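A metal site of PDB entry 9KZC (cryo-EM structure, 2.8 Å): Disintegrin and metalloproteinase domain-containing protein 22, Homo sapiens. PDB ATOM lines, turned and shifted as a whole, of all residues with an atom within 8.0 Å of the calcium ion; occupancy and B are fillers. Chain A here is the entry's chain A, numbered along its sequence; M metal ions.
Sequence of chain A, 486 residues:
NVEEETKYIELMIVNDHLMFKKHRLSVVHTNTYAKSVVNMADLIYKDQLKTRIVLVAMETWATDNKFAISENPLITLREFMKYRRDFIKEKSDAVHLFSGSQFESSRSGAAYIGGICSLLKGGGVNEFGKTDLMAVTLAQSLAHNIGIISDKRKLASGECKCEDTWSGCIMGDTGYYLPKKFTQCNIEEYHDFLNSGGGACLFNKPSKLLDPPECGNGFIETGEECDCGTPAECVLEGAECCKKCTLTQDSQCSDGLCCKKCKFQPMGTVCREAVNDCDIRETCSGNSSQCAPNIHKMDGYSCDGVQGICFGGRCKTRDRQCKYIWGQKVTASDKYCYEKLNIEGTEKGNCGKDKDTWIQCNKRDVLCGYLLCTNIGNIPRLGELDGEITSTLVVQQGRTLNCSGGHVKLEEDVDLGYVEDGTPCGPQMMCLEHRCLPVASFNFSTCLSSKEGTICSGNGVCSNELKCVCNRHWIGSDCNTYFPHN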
ATOM      1  N   SER A 207      16.059  17.681  -8.720  1.00  0.00           N
ATOM      2  CA  SER A 207      15.235  17.533  -9.923  1.00  0.00           C
ATOM      3  C   SER A 207      13.923  18.303  -9.838  1.00  0.00           C
ATOM      4  O   SER A 207      13.450  18.818 -10.855  1.00  0.00           O
ATOM      5  CB  SER A 207      14.939  16.053 -10.181  1.00  0.00           C
ATOM      6  OG  SER A 207      14.217  15.882 -11.389  1.00  0.00           O
ATOM      7  N   LEU A 209      11.897  21.454  -7.782  1.00  0.00           N
ATOM      8  CA  LEU A 209      12.021  22.635  -6.931  1.00  0.00           C
ATOM      9  C   LEU A 209      10.626  23.147  -6.555  1.00  0.00           C
ATOM     10  O   LEU A 209       9.606  22.555  -6.931  1.00  0.00           O
ATOM     11  CB  LEU A 209      12.840  23.708  -7.640  1.00  0.00           C
ATOM     12  CG  LEU A 209      14.380  23.679  -7.615  1.00  0.00           C
ATOM     13  CD1 LEU A 209      14.947  22.343  -8.064  1.00  0.00           C
ATOM     14  CD2 LEU A 209      14.935  24.803  -8.473  1.00  0.00           C
ATOM     15  N   ASP A 211      10.008  26.367  -7.458  1.00  0.00           N
ATOM     16  CA  ASP A 211       9.857  27.444  -8.419  1.00  0.00           C
ATOM     17  C   ASP A 211       9.411  26.898  -9.775  1.00  0.00           C
ATOM     18  O   ASP A 211       9.746  25.759 -10.129  1.00  0.00           O
ATOM     19  CB  ASP A 211      11.175  28.201  -8.593  1.00  0.00           C
ATOM     20  CG  ASP A 211      11.252  29.435  -7.720  1.00  0.00           C
ATOM     21  OD1 ASP A 211      10.196  30.010  -7.389  1.00  0.00           O
ATOM     22  OD2 ASP A 211      12.387  29.844  -7.370  1.00  0.00           O
ATOM     23  N   PRO A 212       8.663  27.684 -10.535  1.00  0.00           N
ATOM     24  CA  PRO A 212       8.346  27.284 -11.905  1.00  0.00           C
ATOM     25  C   PRO A 212       9.613  27.195 -12.725  1.00  0.00           C
ATOM     26  O   PRO A 212      10.596  27.917 -12.465  1.00  0.00           O
ATOM     27  CB  PRO A 212       7.427  28.402 -12.399  1.00  0.00           C
ATOM     28  CG  PRO A 212       6.863  29.011 -11.151  1.00  0.00           C
ATOM     29  CD  PRO A 212       7.959  28.917 -10.143  1.00  0.00           C
ATOM     30  N   PRO A 213       9.645  26.313 -13.728  1.00  0.00           N
ATOM     31  CA  PRO A 213      10.874  26.146 -14.522  1.00  0.00           C
ATOM     32  C   PRO A 213      11.289  27.437 -15.217  1.00  0.00           C
ATOM     33  O   PRO A 213      10.450  28.194 -15.707  1.00  0.00           O
ATOM     34  CB  PRO A 213      10.490  25.059 -15.535  1.00  0.00           C
ATOM     35  CG  PRO A 213       9.340  24.333 -14.911  1.00  0.00           C
ATOM     36  CD  PRO A 213       8.594  25.361 -14.115  1.00  0.00           C
ATOM     37  N   GLU A 214      12.599  27.673 -15.250  1.00  0.00           N
ATOM     38  CA  GLU A 214      13.184  28.776 -15.999  1.00  0.00           C
ATOM     39  C   GLU A 214      14.186  28.215 -16.994  1.00  0.00           C
ATOM     40  O   GLU A 214      14.927  27.284 -16.671  1.00  0.00           O
ATOM     41  CB  GLU A 214      13.871  29.792 -15.076  1.00  0.00           C
ATOM     42  CG  GLU A 214      12.953  30.608 -14.192  1.00  0.00           C
ATOM     43  CD  GLU A 214      12.705  29.953 -12.850  1.00  0.00           C
ATOM     44  OE1 GLU A 214      13.287  28.884 -12.591  1.00  0.00           O
ATOM     45  OE2 GLU A 214      11.923  30.519 -12.056  1.00  0.00           O
ATOM     46  N   CYS A 215      14.203  28.783 -18.198  1.00  0.00           N
ATOM     47  CA  CYS A 215      15.144  28.354 -19.233  1.00  0.00           C
ATOM     48  C   CYS A 215      16.498  29.003 -18.947  1.00  0.00           C
ATOM     49  O   CYS A 215      16.801  30.091 -19.429  1.00  0.00           O
ATOM     50  CB  CYS A 215      14.626  28.726 -20.615  1.00  0.00           C
ATOM     51  SG  CYS A 215      15.583  28.002 -21.966  1.00  0.00           S
ATOM     52  N   GLY A 216      17.309  28.315 -18.150  1.00  0.00           N
ATOM     53  CA  GLY A 216      18.637  28.815 -17.830  1.00  0.00           C
ATOM     54  C   GLY A 216      18.928  28.882 -16.350  1.00  0.00           C
ATOM     55  O   GLY A 216      19.869  29.566 -15.930  1.00  0.00           O
ATOM     56  N   ASN A 217      18.122  28.201 -15.535  1.00  0.00           N
ATOM     57  CA  ASN A 217      18.397  28.157 -14.098  1.00  0.00           C
ATOM     58  C   ASN A 217      19.501  27.162 -13.776  1.00  0.00           C
ATOM     59  O   ASN A 217      20.378  27.449 -12.947  1.00  0.00           O
ATOM     60  CB  ASN A 217      17.114  27.812 -13.332  1.00  0.00           C
ATOM     61  CG  ASN A 217      16.450  26.555 -13.842  1.00  0.00           C
ATOM     62  OD1 ASN A 217      16.810  26.026 -14.892  1.00  0.00           O
ATOM     63  ND2 ASN A 217      15.462  26.066 -13.096  1.00  0.00           N
ATOM     64  N   GLY A 218      19.498  25.999 -14.412  1.00  0.00           N
ATOM     65  CA  GLY A 218      20.557  25.026 -14.217  1.00  0.00           C
ATOM     66  C   GLY A 218      20.060  23.618 -13.933  1.00  0.00           C
ATOM     67  O   GLY A 218      20.781  22.644 -14.173  1.00  0.00           O
ATOM     68  N   PHE A 219      18.839  23.497 -13.428  1.00  0.00           N
ATOM     69  CA  PHE A 219      18.282  22.218 -13.004  1.00  0.00           C
ATOM     70  C   PHE A 219      17.358  21.673 -14.083  1.00  0.00           C
ATOM     71  O   PHE A 219      16.498  22.402 -14.596  1.00  0.00           O
ATOM     72  CB  PHE A 219      17.540  22.359 -11.678  1.00  0.00           C
ATOM     73  CG  PHE A 219      18.320  23.082 -10.618  1.00  0.00           C
ATOM     74  CD1 PHE A 219      19.317  22.427  -9.917  1.00  0.00           C
ATOM     75  CD2 PHE A 219      18.060  24.410 -10.322  1.00  0.00           C
ATOM     76  CE1 PHE A 219      20.041  23.087  -8.943  1.00  0.00           C
ATOM     77  CE2 PHE A 219      18.775  25.067  -9.343  1.00  0.00           C
ATOM     78  CZ  PHE A 219      19.763  24.404  -8.657  1.00  0.00           C
ATOM     79  N   ILE A 220      17.532  20.399 -14.412  1.00  0.00           N
ATOM     80  CA  ILE A 220      16.698  19.728 -15.407  1.00  0.00           C
ATOM     81  C   ILE A 220      15.431  19.247 -14.702  1.00  0.00           C
ATOM     82  O   ILE A 220      15.460  18.265 -13.955  1.00  0.00           O
ATOM     83  CB  ILE A 220      17.441  18.572 -16.092  1.00  0.00           C
ATOM     84  CG1 ILE A 220      18.645  19.079 -16.879  1.00  0.00           C
ATOM     85  CG2 ILE A 220      16.489  17.803 -17.005  1.00  0.00           C
ATOM     86  CD1 ILE A 220      19.938  19.135 -16.089  1.00  0.00           C
ATOM     87  N   GLU A 221      14.325  19.934 -14.940  1.00  0.00           N
ATOM     88  CA  GLU A 221      13.045  19.596 -14.346  1.00  0.00           C
ATOM     89  C   GLU A 221      12.188  18.850 -15.363  1.00  0.00           C
ATOM     90  O   GLU A 221      12.659  18.456 -16.436  1.00  0.00           O
ATOM     91  CB  GLU A 221      12.356  20.863 -13.829  1.00  0.00           C
ATOM     92  CG  GLU A 221      13.101  21.528 -12.679  1.00  0.00           C
ATOM     93  CD  GLU A 221      12.379  22.761 -12.150  1.00  0.00           C
ATOM     94  OE1 GLU A 221      11.368  23.161 -12.765  1.00  0.00           O
ATOM     95  OE2 GLU A 221      12.825  23.319 -11.130  1.00  0.00           O
ATOM     96  N   THR A 222      10.911  18.643 -15.021  1.00  0.00           N
ATOM     97  CA  THR A 222      10.010  17.925 -15.915  1.00  0.00           C
ATOM     98  C   THR A 222       9.851  18.674 -17.236  1.00  0.00           C
ATOM     99  O   THR A 222       9.858  19.911 -17.267  1.00  0.00           O
ATOM    100  CB  THR A 222       8.644  17.729 -15.250  1.00  0.00           C
ATOM    101  OG1 THR A 222       7.775  17.007 -16.133  1.00  0.00           O
ATOM    102  CG2 THR A 222       8.006  19.063 -14.887  1.00  0.00           C
ATOM    103  N   GLU A 224      11.782  19.659 -19.507  1.00  0.00           N
ATOM    104  CA  GLU A 224      13.098  20.045 -19.996  1.00  0.00           C
ATOM    105  C   GLU A 224      14.007  18.838 -20.121  1.00  0.00           C
ATOM    106  O   GLU A 224      14.003  17.943 -19.265  1.00  0.00           O
ATOM    107  CB  GLU A 224      13.733  21.077 -19.053  1.00  0.00           C
ATOM    108  CG  GLU A 224      12.853  22.286 -18.779  1.00  0.00           C
ATOM    109  CD  GLU A 224      13.428  23.183 -17.702  1.00  0.00           C
ATOM    110  OE1 GLU A 224      14.078  22.654 -16.776  1.00  0.00           O
ATOM    111  OE2 GLU A 224      13.237  24.416 -17.786  1.00  0.00           O
ATOM    112  N   CYS A 226      17.555  19.380 -21.365  1.00  0.00           N
ATOM    113  CA  CYS A 226      18.879  19.875 -21.054  1.00  0.00           C
ATOM    114  C   CYS A 226      18.762  21.276 -20.471  1.00  0.00           C
ATOM    115  O   CYS A 226      17.846  22.033 -20.803  1.00  0.00           O
ATOM    116  CB  CYS A 226      19.785  19.903 -22.298  1.00  0.00           C
ATOM    117  SG  CYS A 226      19.185  20.942 -23.650  1.00  0.00           S
ATOM    118  N   ASP A 227      19.715  21.615 -19.586  1.00  0.00           N
ATOM    119  CA  ASP A 227      19.745  22.934 -18.963  1.00  0.00           C
ATOM    120  C   ASP A 227      21.174  23.215 -18.540  1.00  0.00           C
ATOM    121  O   ASP A 227      21.643  22.677 -17.521  1.00  0.00           O
ATOM    122  CB  ASP A 227      18.782  23.010 -17.782  1.00  0.00           C
ATOM    123  CG  ASP A 227      18.238  24.413 -17.562  1.00  0.00           C
ATOM    124  OD1 ASP A 227      19.047  25.365 -17.524  1.00  0.00           O
ATOM    125  OD2 ASP A 227      17.007  24.552 -17.425  1.00  0.00           O
ATOM    126  N   CYS A 245      17.602  25.623 -23.952  1.00  0.00           N
ATOM    127  CA  CYS A 245      16.988  24.517 -23.211  1.00  0.00           C
ATOM    128  C   CYS A 245      16.470  23.433 -24.164  1.00  0.00           C
ATOM    129  O   CYS A 245      15.454  22.794 -23.906  1.00  0.00           O
ATOM    130  CB  CYS A 245      15.877  25.004 -22.292  1.00  0.00           C
ATOM    131  SG  CYS A 245      16.378  26.320 -21.153  1.00  0.00           S
HETATM  132 CA    CA M   1      14.834  24.429 -15.105  1.00  0.00          CA
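N of Glu 221 lies close to OE1 of Glu 224, at 3.3 Å. SG of Cys 215 forms a disulfide with SG of Cys 245, 2.0 Å away. N of Gly 218 sits at hydrogen-bond distance from OD1 of Asp 227 (3.2 Å). OD2 of Asp 227 lies close to OD1 of Asn 217 (2.9 Å). OD1 of Asp 227 sits at hydrogen-bond distance from N of Gly 216, 3.5 Å away. OD1 of Asn 217 sits close to O of Glu 214, 2.9 Å away.
Merely in contact with the calcium ion: Glu 214 (3.3 Å) and Asp 227 (3.2 Å). Of the 18 residues printed, 5 come within 4 Å of the calcium ion. The nearest printed residue that does not touch the calcium ion is Glu 221 (4.2 Å).
The calcium ion is bound by OD1 of Asn 217, OE1 of Glu 224, ND2 of Asn 217 and O of Phe 219. The calcium ion has four donor atoms within binding distance. Slightly farther from the calcium ion lies the side-chain carboxylate (OE2) of Glu 224 (3.1 Å).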
